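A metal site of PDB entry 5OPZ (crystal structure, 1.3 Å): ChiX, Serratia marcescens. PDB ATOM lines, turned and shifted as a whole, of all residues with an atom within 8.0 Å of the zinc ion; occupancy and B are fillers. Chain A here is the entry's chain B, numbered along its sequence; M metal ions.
The backbone NH (N) of Gly 116 lies within hydrogen-bond range of the backbone carbonyl oxygen (O) of His 127, 2.8 Å away. The backbone carbonyl oxygen (O) of His 72 is in hydrogen-bond range of the backbone NH (N) of Arg 51 (3.2 Å). A ring nitrogen (ND1) of His 72 is in hydrogen-bond range of the backbone carbonyl oxygen (O) of Gly 49, at 2.8 Å. The backbone NH (N) of Asp 79 is in hydrogen-bond range of the backbone carbonyl oxygen (O) of Glu 48 (2.8 Å). A ring nitrogen (ND1) of His 72 lies within hydrogen-bond range of the backbone carbonyl oxygen of Ala 77. N of Ser 47 sits at hydrogen-bond distance from O of Asp 79, at 2.8 Å. NE2 of His 127 lies within hydrogen-bond range of OE1 of Gln 129 (2.7 Å). N of His 72 is in hydrogen-bond range of OG of Ser 70.
Three residues have an atom within 4 Å of the zinc ion: His 72, Asp 79 and His 127. The nearest printed residue that does not touch the zinc ion is Arg 51 (4.1 Å).
The zinc ion is bound by the side-chain carboxylate (OD1) of Asp 79 (2.0 Å), a ring nitrogen (ND1) of His 127 (2.0 Å) and a ring nitrogen (NE2) of His 72 (2.1 Å).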
ATOM      1  N   SER A  47      24.944   5.833   3.771  1.00  0.00           N
ATOM      2  CA  SER A  47      25.466   5.952   5.133  1.00  0.00           C
ATOM      3  C   SER A  47      25.572   4.609   5.862  1.00  0.00           C
ATOM      4  O   SER A  47      26.403   4.466   6.752  1.00  0.00           O
ATOM      5  CB  SER A  47      24.672   6.969   5.949  1.00  0.00           C
ATOM      6  OG  SER A  47      23.386   6.477   6.225  1.00  0.00           O
ATOM      7  N   GLU A  48      24.720   3.659   5.493  1.00  0.00           N
ATOM      8  CA  GLU A  48      24.718   2.332   6.115  1.00  0.00           C
ATOM      9  C   GLU A  48      24.164   1.322   5.134  1.00  0.00           C
ATOM     10  O   GLU A  48      23.109   1.528   4.561  1.00  0.00           O
ATOM     11  CB  GLU A  48      23.903   2.347   7.433  1.00  0.00           C
ATOM     12  CG  GLU A  48      24.000   1.036   8.199  1.00  0.00           C
ATOM     13  CD  GLU A  48      23.317   1.030   9.559  1.00  0.00           C
ATOM     14  OE1 GLU A  48      22.371   1.799   9.810  1.00  0.00           O
ATOM     15  OE2 GLU A  48      23.712   0.208  10.400  1.00  0.00           O
ATOM     16  N   GLY A  49      24.919   0.261   4.919  1.00  0.00           N
ATOM     17  CA  GLY A  49      24.483  -0.886   4.134  1.00  0.00           C
ATOM     18  C   GLY A  49      24.326  -2.041   5.080  1.00  0.00           C
ATOM     19  O   GLY A  49      23.304  -2.113   5.789  1.00  0.00           O
ATOM     20  N   ARG A  51      24.619  -3.978   8.497  1.00  0.00           N
ATOM     21  CA  ARG A  51      24.619  -3.600   9.906  1.00  0.00           C
ATOM     22  C   ARG A  51      24.992  -4.824  10.696  1.00  0.00           C
ATOM     23  O   ARG A  51      24.654  -5.930  10.311  1.00  0.00           O
ATOM     24  CB  ARG A  51      23.216  -3.118  10.263  1.00  0.00           C
ATOM     25  CG  ARG A  51      23.002  -2.683  11.714  1.00  0.00           C
ATOM     26  CD  ARG A  51      21.557  -2.339  11.904  1.00  0.00           C
ATOM     27  NE  ARG A  51      21.230  -1.121  11.186  1.00  0.00           N
ATOM     28  CZ  ARG A  51      19.985  -0.707  10.900  1.00  0.00           C
ATOM     29  NH1 ARG A  51      18.924  -1.397  11.267  1.00  0.00           N
ATOM     30  NH2 ARG A  51      19.800   0.438  10.264  1.00  0.00           N
ATOM     31  N   ARG A  55      24.805  -3.810  16.720  1.00  0.00           N
ATOM     32  CA  ARG A  55      24.090  -2.601  16.455  1.00  0.00           C
ATOM     33  C   ARG A  55      22.591  -2.809  16.422  1.00  0.00           C
ATOM     34  O   ARG A  55      21.862  -2.050  17.026  1.00  0.00           O
ATOM     35  CB  ARG A  55      24.602  -1.957  15.150  1.00  0.00           C
ATOM     36  CG  ARG A  55      23.885  -0.698  14.859  1.00  0.00           C
ATOM     37  CD  ARG A  55      24.714   0.163  13.937  1.00  0.00           C
ATOM     38  NE  ARG A  55      23.934   1.038  13.073  1.00  0.00           N
ATOM     39  CZ  ARG A  55      23.229   2.104  13.468  1.00  0.00           C
ATOM     40  NH1 ARG A  55      23.136   2.435  14.738  1.00  0.00           N
ATOM     41  NH2 ARG A  55      22.591   2.833  12.573  1.00  0.00           N
ATOM     42  N   GLN A  56      22.158  -3.874  15.772  1.00  0.00           N
ATOM     43  CA  GLN A  56      20.740  -4.137  15.731  1.00  0.00           C
ATOM     44  C   GLN A  56      20.202  -4.419  17.137  1.00  0.00           C
ATOM     45  O   GLN A  56      19.122  -3.931  17.478  1.00  0.00           O
ATOM     46  CB  GLN A  56      20.398  -5.292  14.790  1.00  0.00           C
ATOM     47  CG  GLN A  56      18.904  -5.424  14.527  1.00  0.00           C
ATOM     48  CD  GLN A  56      18.332  -4.341  13.662  1.00  0.00           C
ATOM     49  OE1 GLN A  56      19.060  -3.724  12.871  1.00  0.00           O
ATOM     50  NE2 GLN A  56      17.034  -4.104  13.767  1.00  0.00           N
ATOM     51  N   MET A  59      19.721  -1.198  18.896  1.00  0.00           N
ATOM     52  CA  MET A  59      18.533  -0.533  18.428  1.00  0.00           C
ATOM     53  C   MET A  59      17.267  -1.092  19.093  1.00  0.00           C
ATOM     54  O   MET A  59      16.368  -0.339  19.439  1.00  0.00           O
ATOM     55  CB  MET A  59      18.412  -0.589  16.904  1.00  0.00           C
ATOM     56  CG  MET A  59      19.488   0.215  16.189  1.00  0.00           C
ATOM     57  SD  MET A  59      19.535  -0.066  14.425  1.00  0.00           S
ATOM     58  CE  MET A  59      17.992   0.708  13.963  1.00  0.00           C
ATOM     59  N   SER A  70      16.287  -7.604  10.495  1.00  0.00           N
ATOM     60  CA  SER A  70      16.430  -6.394   9.690  1.00  0.00           C
ATOM     61  C   SER A  70      16.993  -6.793   8.359  1.00  0.00           C
ATOM     62  O   SER A  70      17.957  -7.552   8.286  1.00  0.00           O
ATOM     63  CB  SER A  70      17.420  -5.441  10.370  1.00  0.00           C
ATOM     64  OG  SER A  70      17.821  -4.376   9.514  1.00  0.00           O
ATOM     65  N   ARG A  71      16.456  -6.164   7.307  1.00  0.00           N
ATOM     66  CA  ARG A  71      16.994  -6.316   6.000  1.00  0.00           C
ATOM     67  C   ARG A  71      18.451  -5.869   5.934  1.00  0.00           C
ATOM     68  O   ARG A  71      19.194  -6.260   5.058  1.00  0.00           O
ATOM     69  CB  ARG A  71      16.125  -5.601   4.996  1.00  0.00           C
ATOM     70  CG  ARG A  71      14.700  -6.098   4.854  1.00  0.00           C
ATOM     71  CD  ARG A  71      14.410  -6.842   3.534  1.00  0.00           C
ATOM     72  NE  ARG A  71      15.025  -8.141   3.521  1.00  0.00           N
ATOM     73  CZ  ARG A  71      14.901  -8.998   2.532  1.00  0.00           C
ATOM     74  NH1 ARG A  71      14.330  -8.639   1.402  1.00  0.00           N
ATOM     75  NH2 ARG A  71      15.382 -10.201   2.674  1.00  0.00           N
ATOM     76  N   HIS A  72      18.877  -4.951   6.818  1.00  0.00           N
ATOM     77  CA  HIS A  72      20.271  -4.513   6.825  1.00  0.00           C
ATOM     78  C   HIS A  72      21.254  -5.572   7.213  1.00  0.00           C
ATOM     79  O   HIS A  72      22.414  -5.527   6.828  1.00  0.00           O
ATOM     80  CB  HIS A  72      20.521  -3.302   7.748  1.00  0.00           C
ATOM     81  CG  HIS A  72      19.992  -1.996   7.246  1.00  0.00           C
ATOM     82  ND1 HIS A  72      20.710  -1.187   6.393  1.00  0.00           N
ATOM     83  CD2 HIS A  72      18.829  -1.364   7.468  1.00  0.00           C
ATOM     84  CE1 HIS A  72      20.028  -0.074   6.170  1.00  0.00           C
ATOM     85  NE2 HIS A  72      18.886  -0.169   6.791  1.00  0.00           N
ATOM     86  N   ALA A  77      19.329  -3.966   2.379  1.00  0.00           N
ATOM     87  CA  ALA A  77      18.886  -2.601   2.615  1.00  0.00           C
ATOM     88  C   ALA A  77      20.061  -1.649   2.667  1.00  0.00           C
ATOM     89  O   ALA A  77      21.158  -2.017   3.044  1.00  0.00           O
ATOM     90  CB  ALA A  77      18.058  -2.483   3.898  1.00  0.00           C
ATOM     91  N   VAL A  78      19.772  -0.390   2.337  1.00  0.00           N
ATOM     92  CA  VAL A  78      20.690   0.688   2.538  1.00  0.00           C
ATOM     93  C   VAL A  78      19.927   1.888   3.105  1.00  0.00           C
ATOM     94  O   VAL A  78      18.761   2.066   2.825  1.00  0.00           O
ATOM     95  CB  VAL A  78      21.351   1.144   1.220  1.00  0.00           C
ATOM     96  CG1 VAL A  78      22.213   0.028   0.631  1.00  0.00           C
ATOM     97  CG2 VAL A  78      20.330   1.610   0.199  1.00  0.00           C
ATOM     98  N   ASP A  79      20.655   2.683   3.890  1.00  0.00           N
ATOM     99  CA  ASP A  79      20.266   4.041   4.233  1.00  0.00           C
ATOM    100  C   ASP A  79      21.135   5.030   3.510  1.00  0.00           C
ATOM    101  O   ASP A  79      22.328   4.925   3.558  1.00  0.00           O
ATOM    102  CB  ASP A  79      20.359   4.254   5.755  1.00  0.00           C
ATOM    103  CG  ASP A  79      19.347   3.431   6.550  1.00  0.00           C
ATOM    104  OD1 ASP A  79      18.453   2.820   6.009  1.00  0.00           O
ATOM    105  OD2 ASP A  79      19.464   3.453   7.797  1.00  0.00           O
ATOM    106  N   VAL A  80      20.508   5.954   2.829  1.00  0.00           N
ATOM    107  CA  VAL A  80      21.221   6.980   2.129  1.00  0.00           C
ATOM    108  C   VAL A  80      21.266   8.273   2.944  1.00  0.00           C
ATOM    109  O   VAL A  80      20.418   8.530   3.812  1.00  0.00           O
ATOM    110  CB  VAL A  80      20.616   7.300   0.742  1.00  0.00           C
ATOM    111  CG1 VAL A  80      20.544   6.050  -0.098  1.00  0.00           C
ATOM    112  CG2 VAL A  80      19.255   7.932   0.834  1.00  0.00           C
ATOM    113  N   GLY A 116      11.428   3.815   2.679  1.00  0.00           N
ATOM    114  CA  GLY A 116      10.901   4.168   3.984  1.00  0.00           C
ATOM    115  C   GLY A 116      10.081   5.418   3.945  1.00  0.00           C
ATOM    116  O   GLY A 116       9.297   5.665   4.869  1.00  0.00           O
ATOM    117  N   TRP A 119       6.647   4.073   4.086  1.00  0.00           N
ATOM    118  CA  TRP A 119       6.184   3.225   5.158  1.00  0.00           C
ATOM    119  C   TRP A 119       4.791   3.664   5.500  1.00  0.00           C
ATOM    120  O   TRP A 119       4.458   4.832   5.354  1.00  0.00           O
ATOM    121  CB  TRP A 119       7.095   3.348   6.390  1.00  0.00           C
ATOM    122  CG  TRP A 119       8.396   2.614   6.273  1.00  0.00           C
ATOM    123  CD1 TRP A 119       8.663   1.553   5.505  1.00  0.00           C
ATOM    124  CD2 TRP A 119       9.601   2.893   6.993  1.00  0.00           C
ATOM    125  NE1 TRP A 119       9.945   1.151   5.676  1.00  0.00           N
ATOM    126  CE2 TRP A 119      10.550   1.958   6.584  1.00  0.00           C
ATOM    127  CE3 TRP A 119       9.968   3.891   7.892  1.00  0.00           C
ATOM    128  CZ2 TRP A 119      11.840   1.946   7.082  1.00  0.00           C
ATOM    129  CZ3 TRP A 119      11.251   3.890   8.385  1.00  0.00           C
ATOM    130  CH2 TRP A 119      12.189   2.936   7.942  1.00  0.00           C
ATOM    131  N   ASP A 124      10.282   7.726   6.909  1.00  0.00           N
ATOM    132  CA  ASP A 124      11.641   8.243   7.035  1.00  0.00           C
ATOM    133  C   ASP A 124      12.365   8.019   5.699  1.00  0.00           C
ATOM    134  O   ASP A 124      12.373   6.944   5.111  1.00  0.00           O
ATOM    135  CB  ASP A 124      12.410   7.598   8.210  1.00  0.00           C
ATOM    136  CG  ASP A 124      13.616   8.410   8.673  1.00  0.00           C
ATOM    137  OD1 ASP A 124      13.522   9.664   8.783  1.00  0.00           O
ATOM    138  OD2 ASP A 124      14.677   7.813   8.968  1.00  0.00           O
ATOM    139  N   PRO A 126      15.685   8.018   4.569  1.00  0.00           N
ATOM    140  CA  PRO A 126      16.925   7.339   4.133  1.00  0.00           C
ATOM    141  C   PRO A 126      16.799   5.882   3.676  1.00  0.00           C
ATOM    142  O   PRO A 126      17.688   5.459   2.912  1.00  0.00           O
ATOM    143  CB  PRO A 126      17.785   7.390   5.384  1.00  0.00           C
ATOM    144  CG  PRO A 126      17.347   8.650   6.059  1.00  0.00           C
ATOM    145  CD  PRO A 126      15.855   8.671   5.881  1.00  0.00           C
ATOM    146  N   HIS A 127      15.772   5.127   4.126  1.00  0.00           N
ATOM    147  CA  HIS A 127      15.803   3.661   4.008  1.00  0.00           C
ATOM    148  C   HIS A 127      15.272   3.178   2.661  1.00  0.00           C
ATOM    149  O   HIS A 127      14.178   3.546   2.276  1.00  0.00           O
ATOM    150  CB  HIS A 127      15.003   3.082   5.133  1.00  0.00           C
ATOM    151  CG  HIS A 127      14.981   1.596   5.169  1.00  0.00           C
ATOM    152  ND1 HIS A 127      15.926   0.863   5.839  1.00  0.00           N
ATOM    153  CD2 HIS A 127      14.129   0.724   4.611  1.00  0.00           C
ATOM    154  CE1 HIS A 127      15.659  -0.413   5.699  1.00  0.00           C
ATOM    155  NE2 HIS A 127      14.572  -0.509   4.945  1.00  0.00           N
ATOM    156  N   PHE A 128      16.045   2.290   2.031  1.00  0.00           N
ATOM    157  CA  PHE A 128      15.604   1.572   0.855  1.00  0.00           C
ATOM    158  C   PHE A 128      15.901   0.076   1.015  1.00  0.00           C
ATOM    159  O   PHE A 128      16.932  -0.257   1.599  1.00  0.00           O
ATOM    160  CB  PHE A 128      16.293   2.035  -0.421  1.00  0.00           C
ATOM    161  CG  PHE A 128      15.964   3.441  -0.811  1.00  0.00           C
ATOM    162  CD1 PHE A 128      16.677   4.508  -0.290  1.00  0.00           C
ATOM    163  CD2 PHE A 128      14.907   3.704  -1.604  1.00  0.00           C
ATOM    164  CE1 PHE A 128      16.382   5.818  -0.638  1.00  0.00           C
ATOM    165  CE2 PHE A 128      14.621   4.992  -2.011  1.00  0.00           C
ATOM    166  CZ  PHE A 128      15.312   6.062  -1.488  1.00  0.00           C
ATOM    167  N   GLN A 129      15.009  -0.798   0.527  1.00  0.00           N
ATOM    168  CA  GLN A 129      15.267  -2.248   0.668  1.00  0.00           C
ATOM    169  C   GLN A 129      14.689  -3.043  -0.468  1.00  0.00           C
ATOM    170  O   GLN A 129      13.691  -2.655  -1.087  1.00  0.00           O
ATOM    171  CB  GLN A 129      14.748  -2.808   1.996  1.00  0.00           C
ATOM    172  CG  GLN A 129      13.235  -2.779   2.121  1.00  0.00           C
ATOM    173  CD  GLN A 129      12.764  -3.266   3.440  1.00  0.00           C
ATOM    174  OE1 GLN A 129      13.275  -2.867   4.475  1.00  0.00           O
ATOM    175  NE2 GLN A 129      11.800  -4.172   3.422  1.00  0.00           N
HETATM  176 ZN    ZN M   1      17.502   1.402   7.014  1.00  0.00          ZN
